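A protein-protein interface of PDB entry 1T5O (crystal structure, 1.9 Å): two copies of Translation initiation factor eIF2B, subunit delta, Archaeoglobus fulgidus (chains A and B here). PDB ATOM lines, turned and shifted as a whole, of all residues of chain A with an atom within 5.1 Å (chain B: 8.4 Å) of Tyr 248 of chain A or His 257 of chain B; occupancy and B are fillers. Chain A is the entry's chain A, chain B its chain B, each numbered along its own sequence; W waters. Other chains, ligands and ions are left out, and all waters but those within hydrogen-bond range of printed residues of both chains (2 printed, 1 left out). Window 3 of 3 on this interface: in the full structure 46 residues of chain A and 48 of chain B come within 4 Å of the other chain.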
ATOM      1  N   GLY A 246      11.343  -5.947  -9.471  1.00  0.00           N
ATOM      2  CA  GLY A 246      12.699  -5.432  -9.417  1.00  0.00           C
ATOM      3  C   GLY A 246      13.677  -6.571  -9.537  1.00  0.00           C
ATOM      4  O   GLY A 246      14.792  -6.401 -10.031  1.00  0.00           O
ATOM      5  N   THR A 247      13.246  -7.746  -9.088  1.00  0.00           N
ATOM      6  CA  THR A 247      14.093  -8.929  -9.136  1.00  0.00           C
ATOM      7  C   THR A 247      14.582  -9.190 -10.565  1.00  0.00           C
ATOM      8  O   THR A 247      15.782  -9.447 -10.779  1.00  0.00           O
ATOM      9  CB  THR A 247      13.338 -10.182  -8.606  1.00  0.00           C
ATOM     10  OG1 THR A 247      12.926  -9.947  -7.259  1.00  0.00           O
ATOM     11  CG2 THR A 247      14.239 -11.408  -8.650  1.00  0.00           C
ATOM     12  N   TYR A 248      13.677  -9.106 -11.534  1.00  0.00           N
ATOM     13  CA  TYR A 248      14.060  -9.343 -12.932  1.00  0.00           C
ATOM     14  C   TYR A 248      15.159  -8.365 -13.357  1.00  0.00           C
ATOM     15  O   TYR A 248      16.150  -8.765 -13.998  1.00  0.00           O
ATOM     16  CB  TYR A 248      12.843  -9.213 -13.883  1.00  0.00           C
ATOM     17  CG  TYR A 248      13.253  -9.134 -15.348  1.00  0.00           C
ATOM     18  CD1 TYR A 248      13.031  -7.965 -16.103  1.00  0.00           C
ATOM     19  CD2 TYR A 248      13.930 -10.193 -15.953  1.00  0.00           C
ATOM     20  CE1 TYR A 248      13.485  -7.870 -17.440  1.00  0.00           C
ATOM     21  CE2 TYR A 248      14.386 -10.111 -17.271  1.00  0.00           C
ATOM     22  CZ  TYR A 248      14.153  -8.940 -18.008  1.00  0.00           C
ATOM     23  OH  TYR A 248      14.575  -8.866 -19.314  1.00  0.00           O
ATOM     24  N   THR A 249      15.003  -7.094 -12.993  1.00  0.00           N
ATOM     25  CA  THR A 249      16.020  -6.097 -13.333  1.00  0.00           C
ATOM     26  C   THR A 249      17.366  -6.526 -12.789  1.00  0.00           C
ATOM     27  O   THR A 249      18.353  -6.479 -13.490  1.00  0.00           O
ATOM     28  CB  THR A 249      15.682  -4.705 -12.741  1.00  0.00           C
ATOM     29  OG1 THR A 249      14.439  -4.272 -13.287  1.00  0.00           O
ATOM     30  CG2 THR A 249      16.767  -3.655 -13.117  1.00  0.00           C
ATOM     31  N   VAL A 250      17.409  -6.897 -11.517  1.00  0.00           N
ATOM     32  CA  VAL A 250      18.659  -7.343 -10.920  1.00  0.00           C
ATOM     33  C   VAL A 250      19.217  -8.528 -11.714  1.00  0.00           C
ATOM     34  O   VAL A 250      20.425  -8.597 -11.968  1.00  0.00           O
ATOM     35  CB  VAL A 250      18.474  -7.775  -9.441  1.00  0.00           C
ATOM     36  CG1 VAL A 250      19.846  -8.304  -8.861  1.00  0.00           C
ATOM     37  CG2 VAL A 250      17.958  -6.588  -8.611  1.00  0.00           C
ATOM     38  N   SER A 251      18.335  -9.439 -12.135  1.00  0.00           N
ATOM     39  CA  SER A 251      18.798 -10.605 -12.892  1.00  0.00           C
ATOM     40  C   SER A 251      19.437 -10.227 -14.243  1.00  0.00           C
ATOM     41  O   SER A 251      20.345 -10.915 -14.720  1.00  0.00           O
ATOM     42  CB  SER A 251      17.649 -11.614 -13.107  1.00  0.00           C
ATOM     43  OG  SER A 251      16.890 -11.323 -14.285  1.00  0.00           O
ATOM     44  N   VAL A 252      18.983  -9.136 -14.852  1.00  0.00           N
ATOM     45  CA  VAL A 252      19.521  -8.743 -16.147  1.00  0.00           C
ATOM     46  C   VAL A 252      20.947  -8.198 -15.978  1.00  0.00           C
ATOM     47  O   VAL A 252      21.834  -8.539 -16.755  1.00  0.00           O
ATOM     48  CB  VAL A 252      18.619  -7.667 -16.828  1.00  0.00           C
ATOM     49  CG1 VAL A 252      19.314  -7.075 -18.099  1.00  0.00           C
ATOM     50  CG2 VAL A 252      17.296  -8.303 -17.245  1.00  0.00           C
ATOM     51  N   ASP A 310       7.558  -9.328 -10.783  1.00  0.00           N
ATOM     52  CA  ASP A 310       7.969  -9.443 -12.165  1.00  0.00           C
ATOM     53  C   ASP A 310       8.456 -10.876 -12.375  1.00  0.00           C
ATOM     54  O   ASP A 310       8.736 -11.594 -11.418  1.00  0.00           O
ATOM     55  CB  ASP A 310       9.039  -8.404 -12.617  1.00  0.00           C
ATOM     56  CG  ASP A 310      10.322  -8.376 -11.765  1.00  0.00           C
ATOM     57  OD1 ASP A 310      10.744  -9.381 -11.149  1.00  0.00           O
ATOM     58  OD2 ASP A 310      10.950  -7.290 -11.770  1.00  0.00           O
ATOM     59  N   PRO A 311       8.491 -11.334 -13.625  1.00  0.00           N
ATOM     60  CA  PRO A 311       8.955 -12.687 -13.922  1.00  0.00           C
ATOM     61  C   PRO A 311      10.421 -12.644 -14.371  1.00  0.00           C
ATOM     62  O   PRO A 311      10.790 -11.850 -15.227  1.00  0.00           O
ATOM     63  CB  PRO A 311       8.030 -13.144 -15.044  1.00  0.00           C
ATOM     64  CG  PRO A 311       7.594 -11.824 -15.750  1.00  0.00           C
ATOM     65  CD  PRO A 311       7.844 -10.689 -14.787  1.00  0.00           C
ATOM     66  N   THR A 312      11.256 -13.462 -13.752  1.00  0.00           N
ATOM     67  CA  THR A 312      12.661 -13.548 -14.130  1.00  0.00           C
ATOM     68  C   THR A 312      12.759 -14.853 -14.942  1.00  0.00           C
ATOM     69  O   THR A 312      12.439 -15.930 -14.420  1.00  0.00           O
ATOM     70  CB  THR A 312      13.595 -13.659 -12.873  1.00  0.00           C
ATOM     71  OG1 THR A 312      13.599 -12.422 -12.146  1.00  0.00           O
ATOM     72  CG2 THR A 312      15.011 -14.002 -13.287  1.00  0.00           C
ATOM     73  N   PRO A 313      13.184 -14.777 -16.221  1.00  0.00           N
ATOM     74  CA  PRO A 313      13.294 -16.009 -17.017  1.00  0.00           C
ATOM     75  C   PRO A 313      14.322 -16.947 -16.379  1.00  0.00           C
ATOM     76  O   PRO A 313      15.347 -16.490 -15.843  1.00  0.00           O
ATOM     77  CB  PRO A 313      13.725 -15.502 -18.396  1.00  0.00           C
ATOM     78  CG  PRO A 313      14.503 -14.224 -18.080  1.00  0.00           C
ATOM     79  CD  PRO A 313      13.697 -13.603 -16.964  1.00  0.00           C
ATOM     80  N   ASN A 316      18.089 -16.712 -16.749  1.00  0.00           N
ATOM     81  CA  ASN A 316      18.891 -15.797 -15.928  1.00  0.00           C
ATOM     82  C   ASN A 316      19.108 -16.344 -14.509  1.00  0.00           C
ATOM     83  O   ASN A 316      19.548 -15.613 -13.621  1.00  0.00           O
ATOM     84  CB  ASN A 316      18.199 -14.432 -15.804  1.00  0.00           C
ATOM     85  CG  ASN A 316      18.196 -13.641 -17.106  1.00  0.00           C
ATOM     86  OD1 ASN A 316      18.523 -14.167 -18.167  1.00  0.00           O
ATOM     87  ND2 ASN A 316      17.797 -12.358 -17.024  1.00  0.00           N
ATOM     88  N   SER B 215      13.244   0.192 -10.264  1.00  0.00           N
ATOM     89  CA  SER B 215      13.387  -1.237 -10.486  1.00  0.00           C
ATOM     90  C   SER B 215      12.428  -1.798 -11.529  1.00  0.00           C
ATOM     91  O   SER B 215      12.641  -2.902 -12.058  1.00  0.00           O
ATOM     92  CB  SER B 215      13.190  -1.980  -9.165  1.00  0.00           C
ATOM     93  OG  SER B 215      11.855  -1.809  -8.722  1.00  0.00           O
ATOM     94  N   MET B 216      11.383  -1.041 -11.841  1.00  0.00           N
ATOM     95  CA  MET B 216      10.403  -1.484 -12.827  1.00  0.00           C
ATOM     96  C   MET B 216      10.856  -1.275 -14.282  1.00  0.00           C
ATOM     97  O   MET B 216      10.114  -1.605 -15.219  1.00  0.00           O
ATOM     98  CB  MET B 216       9.068  -0.783 -12.576  1.00  0.00           C
ATOM     99  CG  MET B 216       8.397  -1.194 -11.273  1.00  0.00           C
ATOM    100  SD  MET B 216       7.008  -0.128 -10.916  1.00  0.00           S
ATOM    101  CE  MET B 216       6.651  -0.620  -9.248  1.00  0.00           C
ATOM    102  N   VAL B 217      12.067  -0.750 -14.489  1.00  0.00           N
ATOM    103  CA  VAL B 217      12.548  -0.572 -15.862  1.00  0.00           C
ATOM    104  C   VAL B 217      12.553  -1.950 -16.525  1.00  0.00           C
ATOM    105  O   VAL B 217      12.282  -2.088 -17.717  1.00  0.00           O
ATOM    106  CB  VAL B 217      14.009   0.058 -15.920  1.00  0.00           C
ATOM    107  CG1 VAL B 217      15.002  -0.793 -15.144  1.00  0.00           C
ATOM    108  CG2 VAL B 217      14.494   0.160 -17.379  1.00  0.00           C
ATOM    109  N   GLY B 218      12.827  -2.983 -15.741  1.00  0.00           N
ATOM    110  CA  GLY B 218      12.855  -4.325 -16.306  1.00  0.00           C
ATOM    111  C   GLY B 218      11.517  -4.826 -16.845  1.00  0.00           C
ATOM    112  O   GLY B 218      11.401  -5.204 -18.017  1.00  0.00           O
ATOM    113  N   ILE B 219      10.480  -4.813 -16.016  1.00  0.00           N
ATOM    114  CA  ILE B 219       9.195  -5.351 -16.467  1.00  0.00           C
ATOM    115  C   ILE B 219       8.554  -4.520 -17.566  1.00  0.00           C
ATOM    116  O   ILE B 219       7.911  -5.039 -18.479  1.00  0.00           O
ATOM    117  CB  ILE B 219       8.221  -5.504 -15.284  1.00  0.00           C
ATOM    118  CG1 ILE B 219       7.082  -6.468 -15.683  1.00  0.00           C
ATOM    119  CG2 ILE B 219       7.746  -4.114 -14.802  1.00  0.00           C
ATOM    120  CD1 ILE B 219       6.007  -6.654 -14.598  1.00  0.00           C
ATOM    121  N   VAL B 220       8.753  -3.209 -17.471  1.00  0.00           N
ATOM    122  CA  VAL B 220       8.198  -2.275 -18.410  1.00  0.00           C
ATOM    123  C   VAL B 220       8.771  -2.550 -19.814  1.00  0.00           C
ATOM    124  O   VAL B 220       8.043  -2.476 -20.799  1.00  0.00           O
ATOM    125  CB  VAL B 220       8.446  -0.860 -17.833  1.00  0.00           C
ATOM    126  CG1 VAL B 220       9.178   0.003 -18.777  1.00  0.00           C
ATOM    127  CG2 VAL B 220       7.150  -0.291 -17.345  1.00  0.00           C
ATOM    128  N   MET B 221      10.048  -2.918 -19.894  1.00  0.00           N
ATOM    129  CA  MET B 221      10.653  -3.262 -21.172  1.00  0.00           C
ATOM    130  C   MET B 221      10.286  -4.685 -21.564  1.00  0.00           C
ATOM    131  O   MET B 221      10.043  -4.964 -22.733  1.00  0.00           O
ATOM    132  CB  MET B 221      12.164  -3.080 -21.127  1.00  0.00           C
ATOM    133  CG  MET B 221      12.543  -1.618 -20.994  1.00  0.00           C
ATOM    134  SD  MET B 221      14.333  -1.297 -21.106  1.00  0.00           S
ATOM    135  CE  MET B 221      14.326   0.433 -20.886  1.00  0.00           C
ATOM    136  N   GLN B 222      10.210  -5.579 -20.588  1.00  0.00           N
ATOM    137  CA  GLN B 222       9.811  -6.957 -20.854  1.00  0.00           C
ATOM    138  C   GLN B 222       8.454  -6.960 -21.551  1.00  0.00           C
ATOM    139  O   GLN B 222       8.209  -7.747 -22.457  1.00  0.00           O
ATOM    140  CB  GLN B 222       9.617  -7.708 -19.563  1.00  0.00           C
ATOM    141  CG  GLN B 222      10.629  -8.714 -19.232  1.00  0.00           C
ATOM    142  CD  GLN B 222      10.215  -9.467 -17.994  1.00  0.00           C
ATOM    143  OE1 GLN B 222       9.246  -9.083 -17.312  1.00  0.00           O
ATOM    144  NE2 GLN B 222      10.938 -10.530 -17.679  1.00  0.00           N
ATOM    145  N   LYS B 223       7.564  -6.083 -21.110  1.00  0.00           N
ATOM    146  CA  LYS B 223       6.233  -6.011 -21.681  1.00  0.00           C
ATOM    147  C   LYS B 223       6.136  -5.098 -22.911  1.00  0.00           C
ATOM    148  O   LYS B 223       5.044  -4.842 -23.396  1.00  0.00           O
ATOM    149  CB  LYS B 223       5.243  -5.524 -20.620  1.00  0.00           C
ATOM    150  CG  LYS B 223       5.207  -6.366 -19.330  1.00  0.00           C
ATOM    151  CD  LYS B 223       4.171  -5.794 -18.349  1.00  0.00           C
ATOM    152  CE  LYS B 223       2.760  -5.919 -18.911  1.00  0.00           C
ATOM    153  NZ  LYS B 223       1.806  -4.959 -18.289  1.00  0.00           N
ATOM    154  N   GLY B 224       7.266  -4.596 -23.402  1.00  0.00           N
ATOM    155  CA  GLY B 224       7.231  -3.721 -24.565  1.00  0.00           C
ATOM    156  C   GLY B 224       6.477  -2.413 -24.396  1.00  0.00           C
ATOM    157  O   GLY B 224       5.932  -1.882 -25.361  1.00  0.00           O
ATOM    158  N   VAL B 226       7.898   0.359 -23.597  1.00  0.00           N
ATOM    159  CA  VAL B 226       8.838   1.431 -23.941  1.00  0.00           C
ATOM    160  C   VAL B 226       9.393   1.332 -25.347  1.00  0.00           C
ATOM    161  O   VAL B 226       9.896   0.293 -25.748  1.00  0.00           O
ATOM    162  CB  VAL B 226      10.046   1.413 -22.963  1.00  0.00           C
ATOM    163  CG1 VAL B 226      11.027   2.506 -23.297  1.00  0.00           C
ATOM    164  CG2 VAL B 226       9.553   1.530 -21.559  1.00  0.00           C
ATOM    165  N   ASP B 227       9.321   2.434 -26.076  1.00  0.00           N
ATOM    166  CA  ASP B 227       9.834   2.499 -27.432  1.00  0.00           C
ATOM    167  C   ASP B 227      11.237   3.074 -27.480  1.00  0.00           C
ATOM    168  O   ASP B 227      12.076   2.635 -28.254  1.00  0.00           O
ATOM    169  CB  ASP B 227       8.903   3.379 -28.274  1.00  0.00           C
ATOM    170  CG  ASP B 227       7.585   2.722 -28.516  1.00  0.00           C
ATOM    171  OD1 ASP B 227       6.549   3.291 -28.134  1.00  0.00           O
ATOM    172  OD2 ASP B 227       7.593   1.608 -29.078  1.00  0.00           O
ATOM    173  N   VAL B 250      19.580   1.380 -16.251  1.00  0.00           N
ATOM    174  CA  VAL B 250      18.582   1.509 -17.319  1.00  0.00           C
ATOM    175  C   VAL B 250      19.234   1.159 -18.658  1.00  0.00           C
ATOM    176  O   VAL B 250      18.636   0.443 -19.465  1.00  0.00           O
ATOM    177  CB  VAL B 250      18.006   2.950 -17.372  1.00  0.00           C
ATOM    178  CG1 VAL B 250      17.019   3.106 -18.547  1.00  0.00           C
ATOM    179  CG2 VAL B 250      17.301   3.250 -16.027  1.00  0.00           C
ATOM    180  N   SER B 251      20.460   1.638 -18.880  1.00  0.00           N
ATOM    181  CA  SER B 251      21.174   1.363 -20.142  1.00  0.00           C
ATOM    182  C   SER B 251      21.421  -0.133 -20.364  1.00  0.00           C
ATOM    183  O   SER B 251      21.381  -0.603 -21.496  1.00  0.00           O
ATOM    184  CB  SER B 251      22.523   2.107 -20.215  1.00  0.00           C
ATOM    185  OG  SER B 251      23.546   1.440 -19.482  1.00  0.00           O
ATOM    186  N   VAL B 252      21.670  -0.884 -19.297  1.00  0.00           N
ATOM    187  CA  VAL B 252      21.880  -2.329 -19.425  1.00  0.00           C
ATOM    188  C   VAL B 252      20.589  -3.026 -19.847  1.00  0.00           C
ATOM    189  O   VAL B 252      20.585  -3.897 -20.740  1.00  0.00           O
ATOM    190  CB  VAL B 252      22.349  -2.947 -18.085  1.00  0.00           C
ATOM    191  CG1 VAL B 252      22.436  -4.492 -18.203  1.00  0.00           C
ATOM    192  CG2 VAL B 252      23.713  -2.368 -17.716  1.00  0.00           C
ATOM    193  N   VAL B 253      19.484  -2.654 -19.221  1.00  0.00           N
ATOM    194  CA  VAL B 253      18.213  -3.293 -19.557  1.00  0.00           C
ATOM    195  C   VAL B 253      17.776  -2.901 -20.987  1.00  0.00           C
ATOM    196  O   VAL B 253      17.337  -3.745 -21.768  1.00  0.00           O
ATOM    197  CB  VAL B 253      17.114  -2.905 -18.530  1.00  0.00           C
ATOM    198  CG1 VAL B 253      15.768  -3.534 -18.901  1.00  0.00           C
ATOM    199  CG2 VAL B 253      17.536  -3.353 -17.127  1.00  0.00           C
ATOM    200  N   ALA B 254      17.889  -1.619 -21.324  1.00  0.00           N
ATOM    201  CA  ALA B 254      17.493  -1.166 -22.651  1.00  0.00           C
ATOM    202  C   ALA B 254      18.314  -1.858 -23.740  1.00  0.00           C
ATOM    203  O   ALA B 254      17.784  -2.246 -24.772  1.00  0.00           O
ATOM    204  CB  ALA B 254      17.649   0.366 -22.764  1.00  0.00           C
ATOM    205  N   LYS B 255      19.605  -1.997 -23.500  1.00  0.00           N
ATOM    206  CA  LYS B 255      20.497  -2.647 -24.453  1.00  0.00           C
ATOM    207  C   LYS B 255      20.054  -4.101 -24.719  1.00  0.00           C
ATOM    208  O   LYS B 255      20.016  -4.566 -25.866  1.00  0.00           O
ATOM    209  CB  LYS B 255      21.893  -2.653 -23.873  1.00  0.00           C
ATOM    210  CG  LYS B 255      22.981  -3.310 -24.709  1.00  0.00           C
ATOM    211  CD  LYS B 255      23.488  -2.368 -25.759  1.00  0.00           C
ATOM    212  CE  LYS B 255      24.862  -2.794 -26.265  1.00  0.00           C
ATOM    213  NZ  LYS B 255      25.193  -2.028 -27.487  1.00  0.00           N
ATOM    214  N   HIS B 256      19.754  -4.819 -23.644  1.00  0.00           N
ATOM    215  CA  HIS B 256      19.329  -6.206 -23.760  1.00  0.00           C
ATOM    216  C   HIS B 256      18.020  -6.322 -24.550  1.00  0.00           C
ATOM    217  O   HIS B 256      17.812  -7.271 -25.320  1.00  0.00           O
ATOM    218  CB  HIS B 256      19.164  -6.820 -22.370  1.00  0.00           C
ATOM    219  CG  HIS B 256      18.725  -8.251 -22.406  1.00  0.00           C
ATOM    220  ND1 HIS B 256      19.549  -9.263 -22.847  1.00  0.00           N
ATOM    221  CD2 HIS B 256      17.523  -8.822 -22.159  1.00  0.00           C
ATOM    222  CE1 HIS B 256      18.872 -10.399 -22.876  1.00  0.00           C
ATOM    223  NE2 HIS B 256      17.638 -10.158 -22.463  1.00  0.00           N
ATOM    224  N   HIS B 257      17.152  -5.328 -24.395  1.00  0.00           N
ATOM    225  CA  HIS B 257      15.869  -5.312 -25.084  1.00  0.00           C
ATOM    226  C   HIS B 257      15.859  -4.583 -26.426  1.00  0.00           C
ATOM    227  O   HIS B 257      14.797  -4.317 -26.996  1.00  0.00           O
ATOM    228  CB  HIS B 257      14.823  -4.730 -24.141  1.00  0.00           C
ATOM    229  CG  HIS B 257      14.391  -5.694 -23.083  1.00  0.00           C
ATOM    230  ND1 HIS B 257      13.445  -6.663 -23.320  1.00  0.00           N
ATOM    231  CD2 HIS B 257      14.850  -5.916 -21.826  1.00  0.00           C
ATOM    232  CE1 HIS B 257      13.340  -7.446 -22.258  1.00  0.00           C
ATOM    233  NE2 HIS B 257      14.181  -7.015 -21.337  1.00  0.00           N
ATOM    234  N   ASN B 258      17.042  -4.232 -26.925  1.00  0.00           N
ATOM    235  CA  ASN B 258      17.142  -3.539 -28.218  1.00  0.00           C
ATOM    236  C   ASN B 258      16.365  -2.234 -28.303  1.00  0.00           C
ATOM    237  O   ASN B 258      15.878  -1.857 -29.369  1.00  0.00           O
ATOM    238  CB  ASN B 258      16.705  -4.480 -29.341  1.00  0.00           C
ATOM    239  CG  ASN B 258      17.660  -5.642 -29.495  1.00  0.00           C
ATOM    240  OD1 ASN B 258      18.854  -5.448 -29.507  1.00  0.00           O
ATOM    241  ND2 ASN B 258      17.132  -6.850 -29.618  1.00  0.00           N
ATOM    242  N   ILE B 259      16.265  -1.540 -27.171  1.00  0.00           N
ATOM    243  CA  ILE B 259      15.558  -0.269 -27.108  1.00  0.00           C
ATOM    244  C   ILE B 259      16.580   0.861 -27.212  1.00  0.00           C
ATOM    245  O   ILE B 259      17.542   0.924 -26.431  1.00  0.00           O
ATOM    246  CB  ILE B 259      14.783  -0.122 -25.775  1.00  0.00           C
ATOM    247  CG1 ILE B 259      13.770  -1.265 -25.650  1.00  0.00           C
ATOM    248  CG2 ILE B 259      14.040   1.234 -25.733  1.00  0.00           C
ATOM    249  CD1 ILE B 259      12.951  -1.215 -24.364  1.00  0.00           C
ATOM    250  N   PRO B 260      16.411   1.737 -28.211  1.00  0.00           N
ATOM    251  CA  PRO B 260      17.316   2.874 -28.415  1.00  0.00           C
ATOM    252  C   PRO B 260      17.521   3.627 -27.094  1.00  0.00           C
ATOM    253  O   PRO B 260      16.562   3.940 -26.386  1.00  0.00           O
ATOM    254  CB  PRO B 260      16.565   3.719 -29.448  1.00  0.00           C
ATOM    255  CG  PRO B 260      15.851   2.677 -30.280  1.00  0.00           C
ATOM    256  CD  PRO B 260      15.337   1.723 -29.225  1.00  0.00           C
HETATM  257  O   HOH W   1      18.965 -10.895 -19.379  1.00  0.00           O
HETATM  258  O   HOH W   2      11.059  -4.838 -13.189  1.00  0.00           O
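The side-chain hydroxyl (OH) of Tyr 248 of chain A is in hydrogen-bond range of a ring nitrogen (NE2) of His 257 of chain B (2.8 Å).
The side-chain hydroxyl (OG1) of Thr 249 of chain A lies within hydrogen-bond range of the backbone carbonyl oxygen (O) of Ser 215 of chain B (2.6 Å).
The side-chain hydroxyl (OG1) of Thr 249 of chain A is in hydrogen-bond range of the backbone NH (N) of Gly 218 of chain B (3.2 Å).
The side-chain amide nitrogen of Gln 222 of chain B is in hydrogen-bond range of the backbone carbonyl oxygen of Pro 311 of chain A (2.8 Å).
3 positions are printed for both chains.
Of the 8 pairs that touch across the chains among the printed residues, none has its exchanged pair printed and touching as well.
Among the printed residues, pairs that only touch across the chains: Tyr 248 of chain A with Gly 218 of chain B, Tyr 248 of chain A with Gln 222 of chain B, Gly 246 of chain A with Ser 215 of chain B and Thr 249 of chain A with Val 217 of chain B.
Tyr 248 of chain A touches three residues of chain B.
Of the printed residues of chain A, Gly 218 of chain B touches Tyr 248 (3.4 Å) and Thr 249 (3.2 Å).
Of the printed residues of chain A, Ser 215 of chain B touches Gly 246 (3.5 Å) and Thr 249 (2.6 Å).
Printed residues of chain B within 4 Å of Gly 246 of chain A: Ser 215 (3.5 Å).
Printed residues of chain B within 4 Å of Pro 311 of chain A: Gln 222 (2.8 Å).
Of the printed residues of chain A, Gln 222 of chain B touches Tyr 248 (3.5 Å) and Pro 311 (2.8 Å).
Lys 223 of chain B touches none of the printed residues of chain A.
The nearest printed residue of chain A that does not touch His 257 of chain B is Val 252 of chain A (5.3 Å).
Water W2 lies within hydrogen-bond range of the backbone carbonyl oxygen (O) of Ser 215 of chain B (2.7 Å), the side-chain carboxylate (OD2) of Asp 310 of chain A (2.8 Å), the backbone NH (N) of Ile 219 of chain B (2.9 Å) and the side-chain hydroxyl (OG1) of Thr 249 of chain A (3.4 Å).
Water W1 bridges ND2 of Asn 316 of chain A and NE2 of His 256 of chain B.
The backbone NH (N) of Tyr 248 of chain A sits close to the side-chain hydroxyl (OG1) of Thr 312 of chain A.
N of Tyr 248 of chain A sits at hydrogen-bond distance from OD1 of Asp 310 of chain A (3.0 Å).
The backbone carbonyl oxygen (O) of Tyr 248 of chain A lies within hydrogen-bond range of the side-chain hydroxyl (OG) of Ser 251 of chain A (2.7 Å).
N of Gly 246 of chain A lies within hydrogen-bond range of OD2 of Asp 310 of chain A (2.7 Å).
Of the 23 printed residues of chain B, 5 touch a printed residue of chain A.
Hydrophobic or aromatic side chains of chain B within 4 Å of the printed part of chain A: Val 217 and His 257.
Of the 12 printed residues of chain A, 4 touch a printed residue of chain B.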
